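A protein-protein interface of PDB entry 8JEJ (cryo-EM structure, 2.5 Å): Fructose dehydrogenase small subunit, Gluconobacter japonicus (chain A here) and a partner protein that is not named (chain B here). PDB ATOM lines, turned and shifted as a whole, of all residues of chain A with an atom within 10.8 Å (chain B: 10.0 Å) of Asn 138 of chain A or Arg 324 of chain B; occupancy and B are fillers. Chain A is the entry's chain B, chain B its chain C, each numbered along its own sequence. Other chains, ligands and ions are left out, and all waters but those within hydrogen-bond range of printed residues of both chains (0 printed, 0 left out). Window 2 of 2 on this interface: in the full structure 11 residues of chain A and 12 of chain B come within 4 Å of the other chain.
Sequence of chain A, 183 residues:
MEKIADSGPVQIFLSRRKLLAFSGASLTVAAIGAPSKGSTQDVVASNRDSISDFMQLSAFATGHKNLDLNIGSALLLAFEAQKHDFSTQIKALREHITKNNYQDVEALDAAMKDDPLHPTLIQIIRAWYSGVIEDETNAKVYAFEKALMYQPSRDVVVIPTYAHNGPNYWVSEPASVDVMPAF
The guanidinium group (NH1) of Arg 324 of chain B lies within hydrogen-bond range of the backbone carbonyl oxygen (O) of Ala 139 of chain A, at 2.9 Å.
The side-chain amide nitrogen (ND2) of Asn 321 of chain B sits at hydrogen-bond distance from the backbone carbonyl oxygen (O) of Val 141 of chain A (2.7 Å).
The backbone carbonyl oxygen (O) of Asn 138 of chain A is in hydrogen-bond range of the guanidinium group (NH2) of Arg 324 of chain B.
Among the printed residues, pairs that only touch across the chains: Lys 140 of chain A with Asn 321 of chain B (3.6 Å), Val 141 of chain A with Val 317 of chain B (3.6 Å), Tyr 142 of chain A with Ala 318 of chain B (3.7 Å), Tyr 142 of chain A with Val 317 of chain B (3.8 Å) and Val 141 of chain A with Ala 318 of chain B (3.8 Å).
Arg 324 of chain B touches just these residues of chain A: Asn 138 (3.2 Å) and Ala 139 (2.9 Å).
Ala 139 of chain A touches just one residue of chain B: Arg 324.
Asn 321 of chain B touches just these residues of chain A: Lys 140 (3.6 Å) and Val 141 (2.7 Å).
No residue of chain A comes within 4 Å of Ser 322 of chain B.
No residue of chain A comes within 4 Å of Ser 325 of chain B.
No residue of chain A comes within 4 Å of Asn 326 of chain B.
Printed residues of chain A within 4 Å of Val 317 of chain B: Val 141 (3.6 Å) and Tyr 142 (3.8 Å).
Of the printed residues of chain A, Ala 318 of chain B touches Val 141 (3.8 Å) and Tyr 142 (3.7 Å).
Printed residues of chain B within 4 Å of Val 141 of chain A: Val 317 (3.6 Å), Ala 318 (3.8 Å) and Asn 321 (2.7 Å).
Of the printed residues of chain B, Lys 140 of chain A touches Asn 321.
The nearest residue of chain B that does not touch Asn 138 of chain A is Asn 321 of chain B (6.5 Å).
Of the 15 printed residues of chain B, 4 touch a printed residue of chain A.
Hydrophobic or aromatic side chains of chain B that line the printed part of chain A: Val 317 and Ala 318.
Of the 14 printed residues of chain A, 5 touch a printed residue of chain B.
Hydrophobic or aromatic side chains of chain A that line the printed part of chain B: Val 141 and Tyr 142.
Among the printed residues, 8 pairs touch across the chains.
Among the printed residues, no Asp or Glu carboxylate lies within 4 Å of a Lys or Arg side-chain nitrogen of the other chain.
N of Tyr 142 of chain A lies within hydrogen-bond range of O of Gly 131 of chain A.
The backbone carbonyl oxygen of Ala 318 of chain B lies within hydrogen-bond range of the side-chain amide nitrogen of Asn 321 of chain B (3.1 Å).
O of Asn 321 of chain B lies within hydrogen-bond range of NE of Arg 324 of chain B (3.2 Å).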
ATOM      1  N   GLY A 131      17.787 -21.731  -9.001  1.00  0.00           N
ATOM      2  CA  GLY A 131      17.450 -20.419  -8.496  1.00  0.00           C
ATOM      3  C   GLY A 131      15.969 -20.117  -8.445  1.00  0.00           C
ATOM      4  O   GLY A 131      15.597 -18.991  -8.095  1.00  0.00           O
ATOM      5  N   VAL A 132      15.113 -21.081  -8.791  1.00  0.00           N
ATOM      6  CA  VAL A 132      13.668 -20.911  -8.746  1.00  0.00           C
ATOM      7  C   VAL A 132      13.053 -22.103  -8.029  1.00  0.00           C
ATOM      8  O   VAL A 132      13.665 -23.165  -7.893  1.00  0.00           O
ATOM      9  CB  VAL A 132      13.040 -20.759 -10.149  1.00  0.00           C
ATOM     10  CG1 VAL A 132      13.502 -19.479 -10.805  1.00  0.00           C
ATOM     11  CG2 VAL A 132      13.368 -21.965 -11.013  1.00  0.00           C
ATOM     12  N   ILE A 133      11.818 -21.912  -7.576  1.00  0.00           N
ATOM     13  CA  ILE A 133      11.057 -22.954  -6.907  1.00  0.00           C
ATOM     14  C   ILE A 133       9.868 -23.409  -7.746  1.00  0.00           C
ATOM     15  O   ILE A 133       9.546 -24.598  -7.777  1.00  0.00           O
ATOM     16  CB  ILE A 133      10.607 -22.477  -5.508  1.00  0.00           C
ATOM     17  CG1 ILE A 133      11.750 -22.635  -4.507  1.00  0.00           C
ATOM     18  CG2 ILE A 133       9.393 -23.244  -5.027  1.00  0.00           C
ATOM     19  CD1 ILE A 133      11.875 -21.486  -3.547  1.00  0.00           C
ATOM     20  N   GLU A 134       9.224 -22.486  -8.452  1.00  0.00           N
ATOM     21  CA  GLU A 134       8.052 -22.804  -9.254  1.00  0.00           C
ATOM     22  C   GLU A 134       8.474 -23.181 -10.672  1.00  0.00           C
ATOM     23  O   GLU A 134       9.656 -23.377 -10.966  1.00  0.00           O
ATOM     24  CB  GLU A 134       7.073 -21.632  -9.246  1.00  0.00           C
ATOM     25  CG  GLU A 134       6.985 -20.903  -7.917  1.00  0.00           C
ATOM     26  CD  GLU A 134       6.026 -21.564  -6.947  1.00  0.00           C
ATOM     27  OE1 GLU A 134       5.971 -22.811  -6.909  1.00  0.00           O
ATOM     28  OE2 GLU A 134       5.324 -20.834  -6.218  1.00  0.00           O
ATOM     29  N   ASP A 135       7.494 -23.289 -11.575  1.00  0.00           N
ATOM     30  CA  ASP A 135       7.742 -23.704 -12.951  1.00  0.00           C
ATOM     31  C   ASP A 135       7.058 -22.789 -13.960  1.00  0.00           C
ATOM     32  O   ASP A 135       6.858 -23.187 -15.111  1.00  0.00           O
ATOM     33  CB  ASP A 135       7.289 -25.150 -13.165  1.00  0.00           C
ATOM     34  CG  ASP A 135       8.362 -26.155 -12.802  1.00  0.00           C
ATOM     35  OD1 ASP A 135       9.539 -25.915 -13.144  1.00  0.00           O
ATOM     36  OD2 ASP A 135       8.031 -27.183 -12.176  1.00  0.00           O
ATOM     37  N   GLU A 136       6.698 -21.576 -13.557  1.00  0.00           N
ATOM     38  CA  GLU A 136       6.038 -20.625 -14.436  1.00  0.00           C
ATOM     39  C   GLU A 136       7.043 -19.620 -14.989  1.00  0.00           C
ATOM     40  O   GLU A 136       8.197 -19.551 -14.561  1.00  0.00           O
ATOM     41  CB  GLU A 136       4.911 -19.900 -13.695  1.00  0.00           C
ATOM     42  CG  GLU A 136       3.705 -20.773 -13.389  1.00  0.00           C
ATOM     43  CD  GLU A 136       3.940 -21.705 -12.217  1.00  0.00           C
ATOM     44  OE1 GLU A 136       3.666 -22.916 -12.354  1.00  0.00           O
ATOM     45  OE2 GLU A 136       4.399 -21.229 -11.159  1.00  0.00           O
ATOM     46  N   THR A 137       6.587 -18.840 -15.966  1.00  0.00           N
ATOM     47  CA  THR A 137       7.407 -17.777 -16.532  1.00  0.00           C
ATOM     48  C   THR A 137       7.472 -16.548 -15.638  1.00  0.00           C
ATOM     49  O   THR A 137       8.264 -15.641 -15.916  1.00  0.00           O
ATOM     50  CB  THR A 137       6.879 -17.379 -17.911  1.00  0.00           C
ATOM     51  OG1 THR A 137       5.687 -16.599 -17.761  1.00  0.00           O
ATOM     52  CG2 THR A 137       6.567 -18.617 -18.741  1.00  0.00           C
ATOM     53  N   ASN A 138       6.658 -16.495 -14.583  1.00  0.00           N
ATOM     54  CA  ASN A 138       6.686 -15.413 -13.609  1.00  0.00           C
ATOM     55  C   ASN A 138       7.173 -15.886 -12.244  1.00  0.00           C
ATOM     56  O   ASN A 138       6.980 -15.189 -11.243  1.00  0.00           O
ATOM     57  CB  ASN A 138       5.300 -14.776 -13.487  1.00  0.00           C
ATOM     58  CG  ASN A 138       5.358 -13.334 -13.021  1.00  0.00           C
ATOM     59  OD1 ASN A 138       6.149 -12.539 -13.527  1.00  0.00           O
ATOM     60  ND2 ASN A 138       4.519 -12.990 -12.050  1.00  0.00           N
ATOM     61  N   ALA A 139       7.789 -17.065 -12.184  1.00  0.00           N
ATOM     62  CA  ALA A 139       8.326 -17.562 -10.926  1.00  0.00           C
ATOM     63  C   ALA A 139       9.432 -16.644 -10.424  1.00  0.00           C
ATOM     64  O   ALA A 139      10.226 -16.113 -11.205  1.00  0.00           O
ATOM     65  CB  ALA A 139       8.858 -18.984 -11.098  1.00  0.00           C
ATOM     66  N   LYS A 140       9.469 -16.445  -9.110  1.00  0.00           N
ATOM     67  CA  LYS A 140      10.480 -15.587  -8.514  1.00  0.00           C
ATOM     68  C   LYS A 140      11.850 -16.248  -8.583  1.00  0.00           C
ATOM     69  O   LYS A 140      11.999 -17.440  -8.305  1.00  0.00           O
ATOM     70  CB  LYS A 140      10.119 -15.270  -7.065  1.00  0.00           C
ATOM     71  CG  LYS A 140       8.900 -14.382  -6.924  1.00  0.00           C
ATOM     72  CD  LYS A 140       8.964 -13.552  -5.658  1.00  0.00           C
ATOM     73  CE  LYS A 140       7.577 -13.102  -5.232  1.00  0.00           C
ATOM     74  NZ  LYS A 140       6.849 -14.168  -4.489  1.00  0.00           N
ATOM     75  N   VAL A 141      12.851 -15.463  -8.962  1.00  0.00           N
ATOM     76  CA  VAL A 141      14.233 -15.920  -9.038  1.00  0.00           C
ATOM     77  C   VAL A 141      14.951 -15.468  -7.777  1.00  0.00           C
ATOM     78  O   VAL A 141      14.936 -14.279  -7.436  1.00  0.00           O
ATOM     79  CB  VAL A 141      14.928 -15.384 -10.301  1.00  0.00           C
ATOM     80  CG1 VAL A 141      16.427 -15.621 -10.230  1.00  0.00           C
ATOM     81  CG2 VAL A 141      14.346 -16.039 -11.540  1.00  0.00           C
ATOM     82  N   TYR A 142      15.568 -16.418  -7.073  1.00  0.00           N
ATOM     83  CA  TYR A 142      16.262 -16.123  -5.831  1.00  0.00           C
ATOM     84  C   TYR A 142      17.775 -16.137  -5.960  1.00  0.00           C
ATOM     85  O   TYR A 142      18.457 -15.637  -5.060  1.00  0.00           O
ATOM     86  CB  TYR A 142      15.835 -17.117  -4.739  1.00  0.00           C
ATOM     87  CG  TYR A 142      14.349 -17.083  -4.482  1.00  0.00           C
ATOM     88  CD1 TYR A 142      13.781 -16.068  -3.728  1.00  0.00           C
ATOM     89  CD2 TYR A 142      13.509 -18.050  -5.019  1.00  0.00           C
ATOM     90  CE1 TYR A 142      12.424 -16.023  -3.501  1.00  0.00           C
ATOM     91  CE2 TYR A 142      12.149 -18.013  -4.797  1.00  0.00           C
ATOM     92  CZ  TYR A 142      11.613 -16.997  -4.037  1.00  0.00           C
ATOM     93  OH  TYR A 142      10.258 -16.951  -3.811  1.00  0.00           O
ATOM     94  N   ALA A 143      18.312 -16.681  -7.048  1.00  0.00           N
ATOM     95  CA  ALA A 143      19.752 -16.709  -7.261  1.00  0.00           C
ATOM     96  C   ALA A 143      20.044 -16.765  -8.751  1.00  0.00           C
ATOM     97  O   ALA A 143      19.544 -17.647  -9.453  1.00  0.00           O
ATOM     98  CB  ALA A 143      20.394 -17.904  -6.551  1.00  0.00           C
ATOM     99  N   PHE A 144      20.844 -15.814  -9.223  1.00  0.00           N
ATOM    100  CA  PHE A 144      21.435 -15.851 -10.551  1.00  0.00           C
ATOM    101  C   PHE A 144      22.909 -15.510 -10.413  1.00  0.00           C
ATOM    102  O   PHE A 144      23.277 -14.648  -9.608  1.00  0.00           O
ATOM    103  CB  PHE A 144      20.752 -14.873 -11.513  1.00  0.00           C
ATOM    104  CG  PHE A 144      21.344 -14.870 -12.893  1.00  0.00           C
ATOM    105  CD1 PHE A 144      21.333 -16.016 -13.669  1.00  0.00           C
ATOM    106  CD2 PHE A 144      21.914 -13.723 -13.415  1.00  0.00           C
ATOM    107  CE1 PHE A 144      21.876 -16.016 -14.937  1.00  0.00           C
ATOM    108  CE2 PHE A 144      22.459 -13.718 -14.682  1.00  0.00           C
ATOM    109  CZ  PHE A 144      22.439 -14.865 -15.443  1.00  0.00           C
ATOM    110  N   VAL B 317      19.116 -10.774  -5.087  1.00  0.00           N
ATOM    111  CA  VAL B 317      18.407 -11.109  -6.317  1.00  0.00           C
ATOM    112  C   VAL B 317      16.908 -11.203  -6.058  1.00  0.00           C
ATOM    113  O   VAL B 317      16.091 -10.827  -6.909  1.00  0.00           O
ATOM    114  CB  VAL B 317      18.968 -12.413  -6.914  1.00  0.00           C
ATOM    115  CG1 VAL B 317      18.197 -12.816  -8.158  1.00  0.00           C
ATOM    116  CG2 VAL B 317      20.439 -12.252  -7.235  1.00  0.00           C
ATOM    117  N   ALA B 318      16.523 -11.704  -4.881  1.00  0.00           N
ATOM    118  CA  ALA B 318      15.108 -11.862  -4.562  1.00  0.00           C
ATOM    119  C   ALA B 318      14.388 -10.519  -4.532  1.00  0.00           C
ATOM    120  O   ALA B 318      13.292 -10.381  -5.091  1.00  0.00           O
ATOM    121  CB  ALA B 318      14.955 -12.584  -3.225  1.00  0.00           C
ATOM    122  N   ASN B 319      14.995  -9.510  -3.904  1.00  0.00           N
ATOM    123  CA  ASN B 319      14.354  -8.206  -3.791  1.00  0.00           C
ATOM    124  C   ASN B 319      14.093  -7.568  -5.149  1.00  0.00           C
ATOM    125  O   ASN B 319      13.252  -6.670  -5.247  1.00  0.00           O
ATOM    126  CB  ASN B 319      15.210  -7.271  -2.938  1.00  0.00           C
ATOM    127  CG  ASN B 319      15.277  -7.704  -1.489  1.00  0.00           C
ATOM    128  OD1 ASN B 319      14.629  -8.671  -1.088  1.00  0.00           O
ATOM    129  ND2 ASN B 319      16.066  -6.993  -0.695  1.00  0.00           N
ATOM    130  N   ALA B 320      14.790  -8.010  -6.193  1.00  0.00           N
ATOM    131  CA  ALA B 320      14.582  -7.476  -7.530  1.00  0.00           C
ATOM    132  C   ALA B 320      13.328  -8.018  -8.202  1.00  0.00           C
ATOM    133  O   ALA B 320      12.890  -7.443  -9.203  1.00  0.00           O
ATOM    134  CB  ALA B 320      15.802  -7.770  -8.406  1.00  0.00           C
ATOM    135  N   ASN B 321      12.737  -9.095  -7.673  1.00  0.00           N
ATOM    136  CA  ASN B 321      11.595  -9.712  -8.339  1.00  0.00           C
ATOM    137  C   ASN B 321      10.393  -8.781  -8.386  1.00  0.00           C
ATOM    138  O   ASN B 321       9.616  -8.819  -9.347  1.00  0.00           O
ATOM    139  CB  ASN B 321      11.223 -11.018  -7.642  1.00  0.00           C
ATOM    140  CG  ASN B 321      12.186 -12.133  -7.959  1.00  0.00           C
ATOM    141  OD1 ASN B 321      12.497 -12.385  -9.120  1.00  0.00           O
ATOM    142  ND2 ASN B 321      12.673 -12.805  -6.925  1.00  0.00           N
ATOM    143  N   SER B 322      10.214  -7.950  -7.360  1.00  0.00           N
ATOM    144  CA  SER B 322       9.135  -6.973  -7.375  1.00  0.00           C
ATOM    145  C   SER B 322       9.318  -5.928  -8.465  1.00  0.00           C
ATOM    146  O   SER B 322       8.335  -5.305  -8.881  1.00  0.00           O
ATOM    147  CB  SER B 322       9.029  -6.287  -6.014  1.00  0.00           C
ATOM    148  OG  SER B 322      10.170  -5.487  -5.762  1.00  0.00           O
ATOM    149  N   ARG B 323      10.544  -5.726  -8.939  1.00  0.00           N
ATOM    150  CA  ARG B 323      10.841  -4.683  -9.910  1.00  0.00           C
ATOM    151  C   ARG B 323      10.783  -5.173 -11.349  1.00  0.00           C
ATOM    152  O   ARG B 323      11.138  -4.420 -12.259  1.00  0.00           O
ATOM    153  CB  ARG B 323      12.209  -4.070  -9.621  1.00  0.00           C
ATOM    154  CG  ARG B 323      12.164  -2.985  -8.570  1.00  0.00           C
ATOM    155  CD  ARG B 323      13.512  -2.327  -8.398  1.00  0.00           C
ATOM    156  NE  ARG B 323      14.604  -3.292  -8.412  1.00  0.00           N
ATOM    157  CZ  ARG B 323      15.203  -3.756  -7.326  1.00  0.00           C
ATOM    158  NH1 ARG B 323      14.809  -3.398  -6.115  1.00  0.00           N
ATOM    159  NH2 ARG B 323      16.223  -4.598  -7.456  1.00  0.00           N
ATOM    160  N   ARG B 324      10.378  -6.417 -11.577  1.00  0.00           N
ATOM    161  CA  ARG B 324      10.048  -6.826 -12.929  1.00  0.00           C
ATOM    162  C   ARG B 324       8.746  -6.154 -13.355  1.00  0.00           C
ATOM    163  O   ARG B 324       7.938  -5.732 -12.522  1.00  0.00           O
ATOM    164  CB  ARG B 324       9.940  -8.347 -13.020  1.00  0.00           C
ATOM    165  CG  ARG B 324      11.205  -9.069 -12.582  1.00  0.00           C
ATOM    166  CD  ARG B 324      11.030 -10.573 -12.603  1.00  0.00           C
ATOM    167  NE  ARG B 324       9.953 -11.005 -11.723  1.00  0.00           N
ATOM    168  CZ  ARG B 324       9.718 -12.265 -11.389  1.00  0.00           C
ATOM    169  NH1 ARG B 324      10.465 -13.254 -11.850  1.00  0.00           N
ATOM    170  NH2 ARG B 324       8.708 -12.541 -10.568  1.00  0.00           N
ATOM    171  N   SER B 325       8.558  -6.040 -14.670  1.00  0.00           N
ATOM    172  CA  SER B 325       7.458  -5.264 -15.246  1.00  0.00           C
ATOM    173  C   SER B 325       7.559  -3.787 -14.870  1.00  0.00           C
ATOM    174  O   SER B 325       6.546  -3.097 -14.746  1.00  0.00           O
ATOM    175  CB  SER B 325       6.091  -5.822 -14.838  1.00  0.00           C
ATOM    176  OG  SER B 325       5.700  -5.304 -13.577  1.00  0.00           O
ATOM    177  N   ASN B 326       8.782  -3.294 -14.697  1.00  0.00           N
ATOM    178  CA  ASN B 326       9.050  -1.939 -14.219  1.00  0.00           C
ATOM    179  C   ASN B 326      10.119  -1.268 -15.064  1.00  0.00           C
ATOM    180  O   ASN B 326      11.098  -0.733 -14.542  1.00  0.00           O
ATOM    181  CB  ASN B 326       9.485  -1.941 -12.759  1.00  0.00           C
ATOM    182  CG  ASN B 326       8.515  -1.220 -11.860  1.00  0.00           C
ATOM    183  OD1 ASN B 326       7.756  -0.359 -12.306  1.00  0.00           O
ATOM    184  ND2 ASN B 326       8.534  -1.565 -10.580  1.00  0.00           N
ATOM    185  N   SER B 327       9.949  -1.287 -16.388  1.00  0.00           N
ATOM    186  CA  SER B 327      10.909  -0.681 -17.310  1.00  0.00           C
ATOM    187  C   SER B 327      11.233   0.762 -16.936  1.00  0.00           C
ATOM    188  O   SER B 327      10.471   1.400 -16.202  1.00  0.00           O
ATOM    189  CB  SER B 327      10.376  -0.737 -18.744  1.00  0.00           C
ATOM    190  OG  SER B 327       9.221   0.068 -18.895  1.00  0.00           O
ATOM    191  N   THR B 328      12.371   1.268 -17.417  1.00  0.00           N
ATOM    192  CA  THR B 328      12.877   2.617 -17.130  1.00  0.00           C
ATOM    193  C   THR B 328      12.974   2.856 -15.615  1.00  0.00           C
ATOM    194  O   THR B 328      12.238   3.629 -15.002  1.00  0.00           O
ATOM    195  CB  THR B 328      12.088   3.694 -17.911  1.00  0.00           C
ATOM    196  OG1 THR B 328      12.918   4.846 -18.112  1.00  0.00           O
ATOM    197  CG2 THR B 328      10.745   4.126 -17.295  1.00  0.00           C
ATOM    198  N   LEU B 329      13.936   2.139 -15.022  1.00  0.00           N
ATOM    199  CA  LEU B 329      14.108   2.097 -13.571  1.00  0.00           C
ATOM    200  C   LEU B 329      14.038   3.473 -12.922  1.00  0.00           C
ATOM    201  O   LEU B 329      14.866   4.352 -13.180  1.00  0.00           O
ATOM    202  CB  LEU B 329      15.432   1.410 -13.197  1.00  0.00           C
ATOM    203  CG  LEU B 329      16.830   1.805 -13.697  1.00  0.00           C
ATOM    204  CD1 LEU B 329      17.470   2.897 -12.863  1.00  0.00           C
ATOM    205  CD2 LEU B 329      17.724   0.582 -13.679  1.00  0.00           C
ATOM    206  N   LYS B 331      11.900   3.241  -9.755  1.00  0.00           N
ATOM    207  CA  LYS B 331      11.600   2.619  -8.474  1.00  0.00           C
ATOM    208  C   LYS B 331      12.779   1.840  -7.911  1.00  0.00           C
ATOM    209  O   LYS B 331      12.653   1.247  -6.835  1.00  0.00           O
ATOM    210  CB  LYS B 331      10.386   1.696  -8.611  1.00  0.00           C
ATOM    211  CG  LYS B 331       9.245   2.290  -9.418  1.00  0.00           C
ATOM    212  CD  LYS B 331       7.899   1.939  -8.810  1.00  0.00           C
ATOM    213  CE  LYS B 331       6.826   1.792  -9.876  1.00  0.00           C
ATOM    214  NZ  LYS B 331       7.147   2.570 -11.104  1.00  0.00           N
ATOM    215  N   THR B 332      13.907   1.810  -8.616  1.00  0.00           N
ATOM    216  CA  THR B 332      15.136   1.216  -8.098  1.00  0.00           C
ATOM    217  C   THR B 332      15.919   2.317  -7.395  1.00  0.00           C
ATOM    218  O   THR B 332      16.628   3.098  -8.032  1.00  0.00           O
ATOM    219  CB  THR B 332      15.954   0.579  -9.215  1.00  0.00           C
ATOM    220  OG1 THR B 332      15.083  -0.119 -10.113  1.00  0.00           O
ATOM    221  CG2 THR B 332      16.962  -0.398  -8.636  1.00  0.00           C
